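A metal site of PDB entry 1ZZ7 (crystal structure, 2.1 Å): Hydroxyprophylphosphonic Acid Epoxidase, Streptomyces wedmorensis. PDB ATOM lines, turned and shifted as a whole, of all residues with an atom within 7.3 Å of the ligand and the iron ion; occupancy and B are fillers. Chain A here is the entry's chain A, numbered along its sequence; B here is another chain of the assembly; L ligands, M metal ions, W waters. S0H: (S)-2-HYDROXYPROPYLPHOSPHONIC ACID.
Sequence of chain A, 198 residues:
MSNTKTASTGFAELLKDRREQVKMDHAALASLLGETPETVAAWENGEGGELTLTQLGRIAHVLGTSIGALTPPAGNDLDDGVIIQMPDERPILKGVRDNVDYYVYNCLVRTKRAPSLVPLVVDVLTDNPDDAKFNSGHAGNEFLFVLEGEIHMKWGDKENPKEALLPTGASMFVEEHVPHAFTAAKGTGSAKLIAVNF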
ATOM      1  N   TYR A 103      11.602 -28.653  11.521  1.00  0.00           N
ATOM      2  CA  TYR A 103      10.455 -29.538  11.240  1.00  0.00           C
ATOM      3  C   TYR A 103      10.716 -30.449  10.050  1.00  0.00           C
ATOM      4  O   TYR A 103      11.207 -29.999   9.009  1.00  0.00           O
ATOM      5  CB  TYR A 103       9.203 -28.737  10.902  1.00  0.00           C
ATOM      6  CG  TYR A 103       8.893 -27.633  11.857  1.00  0.00           C
ATOM      7  CD1 TYR A 103       9.432 -26.358  11.683  1.00  0.00           C
ATOM      8  CD2 TYR A 103       8.062 -27.863  12.967  1.00  0.00           C
ATOM      9  CE1 TYR A 103       9.169 -25.324  12.591  1.00  0.00           C
ATOM     10  CE2 TYR A 103       7.793 -26.850  13.885  1.00  0.00           C
ATOM     11  CZ  TYR A 103       8.344 -25.582  13.683  1.00  0.00           C
ATOM     12  OH  TYR A 103       8.067 -24.559  14.581  1.00  0.00           O
ATOM     13  N   TYR A 105       8.608 -33.040   7.637  1.00  0.00           N
ATOM     14  CA  TYR A 105       7.279 -33.516   7.292  1.00  0.00           C
ATOM     15  C   TYR A 105       7.325 -34.857   6.579  1.00  0.00           C
ATOM     16  O   TYR A 105       7.996 -34.996   5.574  1.00  0.00           O
ATOM     17  CB  TYR A 105       6.567 -32.492   6.396  1.00  0.00           C
ATOM     18  CG  TYR A 105       6.561 -31.093   6.957  1.00  0.00           C
ATOM     19  CD1 TYR A 105       7.678 -30.263   6.845  1.00  0.00           C
ATOM     20  CD2 TYR A 105       5.448 -30.603   7.657  1.00  0.00           C
ATOM     21  CE1 TYR A 105       7.696 -28.988   7.422  1.00  0.00           C
ATOM     22  CE2 TYR A 105       5.460 -29.332   8.229  1.00  0.00           C
ATOM     23  CZ  TYR A 105       6.584 -28.525   8.111  1.00  0.00           C
ATOM     24  OH  TYR A 105       6.605 -27.264   8.679  1.00  0.00           O
ATOM     25  N   LEU A 120      -0.104 -35.577   7.376  1.00  0.00           N
ATOM     26  CA  LEU A 120       1.333 -35.574   7.636  1.00  0.00           C
ATOM     27  C   LEU A 120       1.711 -36.039   9.045  1.00  0.00           C
ATOM     28  O   LEU A 120       0.926 -35.921   9.986  1.00  0.00           O
ATOM     29  CB  LEU A 120       1.869 -34.143   7.499  1.00  0.00           C
ATOM     30  CG  LEU A 120       1.598 -33.282   6.263  1.00  0.00           C
ATOM     31  CD1 LEU A 120       1.865 -31.811   6.601  1.00  0.00           C
ATOM     32  CD2 LEU A 120       2.475 -33.734   5.112  1.00  0.00           C
ATOM     33  N   VAL A 122       4.417 -34.979  11.579  1.00  0.00           N
ATOM     34  CA  VAL A 122       5.411 -33.910  11.737  1.00  0.00           C
ATOM     35  C   VAL A 122       6.312 -34.156  12.948  1.00  0.00           C
ATOM     36  O   VAL A 122       5.838 -34.377  14.062  1.00  0.00           O
ATOM     37  CB  VAL A 122       4.730 -32.524  11.934  1.00  0.00           C
ATOM     38  CG1 VAL A 122       5.776 -31.415  11.885  1.00  0.00           C
ATOM     39  CG2 VAL A 122       3.672 -32.279  10.854  1.00  0.00           C
ATOM     40  N   LYS A 133       6.999 -19.868  14.502  1.00  0.00           N
ATOM     41  CA  LYS A 133       6.725 -18.895  13.448  1.00  0.00           C
ATOM     42  C   LYS A 133       5.319 -19.148  12.935  1.00  0.00           C
ATOM     43  O   LYS A 133       5.021 -20.206  12.387  1.00  0.00           O
ATOM     44  CB  LYS A 133       7.739 -19.021  12.306  1.00  0.00           C
ATOM     45  N   PHE A 134       4.439 -18.159  13.104  1.00  0.00           N
ATOM     46  CA  PHE A 134       3.051 -18.309  12.675  1.00  0.00           C
ATOM     47  C   PHE A 134       2.777 -18.433  11.188  1.00  0.00           C
ATOM     48  O   PHE A 134       3.503 -17.881  10.355  1.00  0.00           O
ATOM     49  CB  PHE A 134       2.214 -17.145  13.174  1.00  0.00           C
ATOM     50  CG  PHE A 134       1.693 -17.317  14.556  1.00  0.00           C
ATOM     51  CD1 PHE A 134       2.522 -17.150  15.652  1.00  0.00           C
ATOM     52  CD2 PHE A 134       0.348 -17.628  14.767  1.00  0.00           C
ATOM     53  CE1 PHE A 134       2.031 -17.291  16.941  1.00  0.00           C
ATOM     54  CE2 PHE A 134      -0.149 -17.774  16.050  1.00  0.00           C
ATOM     55  CZ  PHE A 134       0.689 -17.594  17.140  1.00  0.00           C
ATOM     56  N   ASN A 135       1.690 -19.139  10.876  1.00  0.00           N
ATOM     57  CA  ASN A 135       1.201 -19.317   9.515  1.00  0.00           C
ATOM     58  C   ASN A 135       0.449 -18.036   9.250  1.00  0.00           C
ATOM     59  O   ASN A 135       0.590 -17.048   9.961  1.00  0.00           O
ATOM     60  CB  ASN A 135       0.156 -20.428   9.449  1.00  0.00           C
ATOM     61  CG  ASN A 135       0.725 -21.738   9.027  1.00  0.00           C
ATOM     62  OD1 ASN A 135       1.715 -21.784   8.285  1.00  0.00           O
ATOM     63  ND2 ASN A 135       0.105 -22.820   9.482  1.00  0.00           N
ATOM     64  N   SER A 136      -0.400 -18.088   8.219  1.00  0.00           N
ATOM     65  CA  SER A 136      -1.255 -16.967   7.883  1.00  0.00           C
ATOM     66  C   SER A 136      -2.622 -17.615   7.805  1.00  0.00           C
ATOM     67  O   SER A 136      -3.619 -16.961   7.516  1.00  0.00           O
ATOM     68  CB  SER A 136      -0.869 -16.383   6.529  1.00  0.00           C
ATOM     69  OG  SER A 136      -1.030 -17.358   5.517  1.00  0.00           O
ATOM     70  N   GLY A 137      -2.660 -18.928   8.078  1.00  0.00           N
ATOM     71  CA  GLY A 137      -3.898 -19.680   8.034  1.00  0.00           C
ATOM     72  C   GLY A 137      -3.936 -20.628   6.850  1.00  0.00           C
ATOM     73  O   GLY A 137      -3.200 -20.442   5.873  1.00  0.00           O
ATOM     74  N   HIS A 138      -4.795 -21.641   6.926  1.00  0.00           N
ATOM     75  CA  HIS A 138      -4.947 -22.619   5.846  1.00  0.00           C
ATOM     76  C   HIS A 138      -6.276 -22.488   5.187  1.00  0.00           C
ATOM     77  O   HIS A 138      -7.241 -21.957   5.745  1.00  0.00           O
ATOM     78  CB  HIS A 138      -4.941 -24.068   6.357  1.00  0.00           C
ATOM     79  CG  HIS A 138      -3.665 -24.496   6.983  1.00  0.00           C
ATOM     80  ND1 HIS A 138      -2.440 -24.036   6.562  1.00  0.00           N
ATOM     81  CD2 HIS A 138      -3.420 -25.378   7.981  1.00  0.00           C
ATOM     82  CE1 HIS A 138      -1.485 -24.601   7.286  1.00  0.00           C
ATOM     83  NE2 HIS A 138      -2.060 -25.422   8.157  1.00  0.00           N
ATOM     84  N   GLU A 142      -8.160 -28.395   9.886  1.00  0.00           N
ATOM     85  CA  GLU A 142      -7.032 -29.243  10.243  1.00  0.00           C
ATOM     86  C   GLU A 142      -7.222 -29.968  11.560  1.00  0.00           C
ATOM     87  O   GLU A 142      -7.562 -29.379  12.581  1.00  0.00           O
ATOM     88  CB  GLU A 142      -5.740 -28.408  10.286  1.00  0.00           C
ATOM     89  CG  GLU A 142      -4.465 -29.225  10.591  1.00  0.00           C
ATOM     90  CD  GLU A 142      -3.200 -28.380  10.443  1.00  0.00           C
ATOM     91  OE1 GLU A 142      -2.091 -28.882  10.720  1.00  0.00           O
ATOM     92  OE2 GLU A 142      -3.312 -27.216  10.034  1.00  0.00           O
ATOM     93  N   LEU A 144      -5.360 -32.419  14.381  1.00  0.00           N
ATOM     94  CA  LEU A 144      -4.026 -32.787  14.869  1.00  0.00           C
ATOM     95  C   LEU A 144      -4.103 -33.756  16.051  1.00  0.00           C
ATOM     96  O   LEU A 144      -5.057 -33.728  16.824  1.00  0.00           O
ATOM     97  CB  LEU A 144      -3.218 -31.550  15.276  1.00  0.00           C
ATOM     98  CG  LEU A 144      -2.861 -30.549  14.176  1.00  0.00           C
ATOM     99  CD1 LEU A 144      -4.010 -29.561  13.998  1.00  0.00           C
ATOM    100  CD2 LEU A 144      -1.584 -29.796  14.560  1.00  0.00           C
ATOM    101  N   VAL A 174      -8.351 -27.143  14.160  1.00  0.00           N
ATOM    102  CA  VAL A 174      -8.080 -25.768  13.788  1.00  0.00           C
ATOM    103  C   VAL A 174      -8.922 -25.418  12.565  1.00  0.00           C
ATOM    104  O   VAL A 174      -8.742 -25.995  11.492  1.00  0.00           O
ATOM    105  CB  VAL A 174      -6.590 -25.533  13.442  1.00  0.00           C
ATOM    106  CG1 VAL A 174      -6.346 -24.040  13.180  1.00  0.00           C
ATOM    107  CG2 VAL A 174      -5.702 -26.023  14.570  1.00  0.00           C
ATOM    108  N   VAL A 178      -7.472 -19.950  10.330  1.00  0.00           N
ATOM    109  CA  VAL A 178      -6.919 -19.556  11.636  1.00  0.00           C
ATOM    110  C   VAL A 178      -5.396 -19.764  11.647  1.00  0.00           C
ATOM    111  O   VAL A 178      -4.917 -20.889  11.525  1.00  0.00           O
ATOM    112  CB  VAL A 178      -7.516 -20.394  12.788  1.00  0.00           C
ATOM    113  CG1 VAL A 178      -6.883 -19.959  14.104  1.00  0.00           C
ATOM    114  CG2 VAL A 178      -9.038 -20.214  12.845  1.00  0.00           C
ATOM    115  N   HIS A 180      -1.655 -20.398  12.889  1.00  0.00           N
ATOM    116  CA  HIS A 180      -1.127 -21.138  14.029  1.00  0.00           C
ATOM    117  C   HIS A 180       0.357 -21.449  13.925  1.00  0.00           C
ATOM    118  O   HIS A 180       0.963 -21.285  12.870  1.00  0.00           O
ATOM    119  CB  HIS A 180      -1.923 -22.440  14.242  1.00  0.00           C
ATOM    120  CG  HIS A 180      -1.999 -23.303  13.021  1.00  0.00           C
ATOM    121  ND1 HIS A 180      -2.728 -22.952  11.902  1.00  0.00           N
ATOM    122  CD2 HIS A 180      -1.417 -24.491  12.730  1.00  0.00           C
ATOM    123  CE1 HIS A 180      -2.576 -23.879  10.974  1.00  0.00           C
ATOM    124  NE2 HIS A 180      -1.790 -24.818  11.447  1.00  0.00           N
ATOM    125  N   ALA A 181       0.931 -21.890  15.028  1.00  0.00           N
ATOM    126  CA  ALA A 181       2.352 -22.249  15.095  1.00  0.00           C
ATOM    127  C   ALA A 181       2.562 -23.157  16.285  1.00  0.00           C
ATOM    128  O   ALA A 181       1.754 -23.171  17.218  1.00  0.00           O
ATOM    129  CB  ALA A 181       3.222 -20.997  15.229  1.00  0.00           C
ATOM    130  N   PHE A 182       3.620 -23.944  16.259  1.00  0.00           N
ATOM    131  CA  PHE A 182       3.884 -24.813  17.375  1.00  0.00           C
ATOM    132  C   PHE A 182       5.317 -25.316  17.399  1.00  0.00           C
ATOM    133  O   PHE A 182       5.997 -25.344  16.366  1.00  0.00           O
ATOM    134  CB  PHE A 182       2.923 -26.008  17.382  1.00  0.00           C
ATOM    135  CG  PHE A 182       2.953 -26.809  16.113  1.00  0.00           C
ATOM    136  CD1 PHE A 182       1.985 -26.609  15.136  1.00  0.00           C
ATOM    137  CD2 PHE A 182       3.939 -27.758  15.899  1.00  0.00           C
ATOM    138  CE1 PHE A 182       2.006 -27.350  13.933  1.00  0.00           C
ATOM    139  CE2 PHE A 182       3.985 -28.514  14.718  1.00  0.00           C
ATOM    140  CZ  PHE A 182       3.014 -28.311  13.723  1.00  0.00           C
ATOM    141  N   LEU A 193       3.710 -35.172  15.994  1.00  0.00           N
ATOM    142  CA  LEU A 193       2.273 -35.110  15.884  1.00  0.00           C
ATOM    143  C   LEU A 193       1.820 -35.451  14.487  1.00  0.00           C
ATOM    144  O   LEU A 193       2.582 -35.308  13.521  1.00  0.00           O
ATOM    145  CB  LEU A 193       1.775 -33.708  16.253  1.00  0.00           C
ATOM    146  CG  LEU A 193       2.239 -32.541  15.369  1.00  0.00           C
ATOM    147  CD1 LEU A 193       1.471 -32.523  14.039  1.00  0.00           C
ATOM    148  CD2 LEU A 193       2.018 -31.253  16.113  1.00  0.00           C
ATOM    149  N   ALA A 195      -0.783 -34.487  11.564  1.00  0.00           N
ATOM    150  CA  ALA A 195      -1.630 -33.370  11.182  1.00  0.00           C
ATOM    151  C   ALA A 195      -2.364 -33.698   9.891  1.00  0.00           C
ATOM    152  O   ALA A 195      -1.740 -34.022   8.887  1.00  0.00           O
ATOM    153  CB  ALA A 195      -0.803 -32.107  11.010  1.00  0.00           C
ATOM    154  N   ASN A 197      -4.859 -32.116   7.164  1.00  0.00           N
ATOM    155  CA  ASN A 197      -5.579 -30.992   6.588  1.00  0.00           C
ATOM    156  C   ASN A 197      -6.642 -31.598   5.671  1.00  0.00           C
ATOM    157  O   ASN A 197      -6.334 -32.485   4.865  1.00  0.00           O
ATOM    158  CB  ASN A 197      -4.614 -30.103   5.795  1.00  0.00           C
ATOM    159  CG  ASN A 197      -3.848 -29.131   6.691  1.00  0.00           C
ATOM    160  OD1 ASN A 197      -4.401 -28.135   7.161  1.00  0.00           O
ATOM    161  ND2 ASN A 197      -2.599 -29.436   6.950  1.00  0.00           N
ATOM    162  N   GLU B  20       2.867 -25.119  -1.523  1.00  0.00           N
ATOM    163  CA  GLU B  20       3.130 -24.979  -0.097  1.00  0.00           C
ATOM    164  C   GLU B  20       2.242 -25.931   0.660  1.00  0.00           C
ATOM    165  O   GLU B  20       2.629 -26.490   1.684  1.00  0.00           O
ATOM    166  CB  GLU B  20       2.864 -23.550   0.367  1.00  0.00           C
ATOM    167  CG  GLU B  20       4.030 -22.627   0.094  1.00  0.00           C
ATOM    168  CD  GLU B  20       3.690 -21.153   0.277  1.00  0.00           C
ATOM    169  OE1 GLU B  20       4.608 -20.326   0.120  1.00  0.00           O
ATOM    170  OE2 GLU B  20       2.506 -20.830   0.558  1.00  0.00           O
ATOM    171  N   GLN B  21       1.035 -26.113   0.161  1.00  0.00           N
ATOM    172  CA  GLN B  21       0.082 -26.995   0.795  1.00  0.00           C
ATOM    173  C   GLN B  21       0.593 -28.434   0.839  1.00  0.00           C
ATOM    174  O   GLN B  21       0.344 -29.142   1.824  1.00  0.00           O
ATOM    175  CB  GLN B  21      -1.263 -26.905   0.061  1.00  0.00           C
ATOM    176  CG  GLN B  21      -2.444 -27.433   0.847  1.00  0.00           C
ATOM    177  CD  GLN B  21      -3.742 -27.333   0.060  1.00  0.00           C
ATOM    178  OE1 GLN B  21      -4.784 -27.848   0.492  1.00  0.00           O
ATOM    179  NE2 GLN B  21      -3.688 -26.702  -1.115  1.00  0.00           N
ATOM    180  N   LYS B  23       3.768 -29.322   0.921  1.00  0.00           N
ATOM    181  CA  LYS B  23       5.138 -29.336   1.425  1.00  0.00           C
ATOM    182  C   LYS B  23       6.203 -29.561   0.357  1.00  0.00           C
ATOM    183  O   LYS B  23       7.119 -30.374   0.527  1.00  0.00           O
ATOM    184  CB  LYS B  23       5.263 -30.411   2.508  1.00  0.00           C
ATOM    185  CG  LYS B  23       4.294 -30.215   3.655  1.00  0.00           C
ATOM    186  CD  LYS B  23       4.458 -28.830   4.199  1.00  0.00           C
ATOM    187  CE  LYS B  23       3.353 -28.469   5.160  1.00  0.00           C
ATOM    188  NZ  LYS B  23       3.467 -27.016   5.505  1.00  0.00           N
HETATM  189  P1  S0H L   1       1.997 -25.718   8.767  1.00  0.00           P
HETATM  190  C2  S0H L   1       3.094 -24.542   9.657  1.00  0.00           C
HETATM  191  C3  S0H L   1       3.978 -23.720   8.687  1.00  0.00           C
HETATM  192  O6  S0H L   1       4.563 -22.631   9.389  1.00  0.00           O
HETATM  193  C1  S0H L   1       4.822 -24.339   8.321  1.00  0.00           C
HETATM  194  O13 S0H L   1       2.031 -25.599   7.304  1.00  0.00           O
HETATM  195  O14 S0H L   1       0.545 -25.539   9.318  1.00  0.00           O
HETATM  196  O15 S0H L   1       2.235 -27.178   9.313  1.00  0.00           O
HETATM  197 FE    FE M   1      -1.475 -26.091   9.697  1.00  0.00          FE
HETATM  198  O   HOH W   1      -0.524 -27.129  11.368  1.00  0.00           O
HETATM  199  O   HOH W   2      -0.538 -28.012   8.202  1.00  0.00           O
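OE2 of Glu 142 sits close to OD1 of Asn 197, at 3.2 Å.
The backbone carbonyl oxygen (O) of Glu 142 is in hydrogen-bond range of the backbone NH (N) of Val 174 (2.8 Å).
N of Asn 135 sits at hydrogen-bond distance from O of His 180, 3.0 Å away.
O of Val 178 lies within hydrogen-bond range of ND1 of His 180 (3.0 Å).
Water W1 lies within hydrogen-bond range of OE1 of Glu 142 (2.4 Å) and O15 of the ligand (3.4 Å).
Water W2 lies within hydrogen-bond range of the side-chain amide nitrogen of Asn 197 (2.8 Å), the side-chain carboxylate of Glu 142 (3.1 Å) and an oxygen (O15) of the ligand (3.1 Å).
Merely in contact with the ligand: Tyr 105 and Lys 133.
Hydrophobic or aromatic side chains within 4 Å of the ligand: His 138 and His 180.
Within 4 Å of the ligand: Tyr 105, Lys 133, Asn 135, His 138, His 180 and Lys 23 of chain B.
An oxygen (O13) of the ligand lies within salt-bridge range of the side-chain amino group (NZ) of Lys 23 of chain B (2.7 Å).
The side-chain amide oxygen (OD1) of Asn 135 lies close to an oxygen (O6) of the ligand.
The iron ion is bound by NE2 of His 138 (1.8 Å).
The iron ion is bound by an oxygen (O14) of the ligand, at 2.1 Å.
The iron ion is bound by the side-chain carboxylate (OE2) of Glu 142, at 2.2 Å.
The iron ion is bound by water W1, 2.2 Å away.
The iron ion is bound by a ring nitrogen (NE2) of His 180, 2.2 Å away.
Slightly farther from the iron ion lies water W2 (2.6 Å).
Asn 135 touches the iron ion (ND2 to FE, 3.6 Å).
Four residues have an atom within 4 Å of the iron ion: Asn 135, His 138, Glu 142 and His 180.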
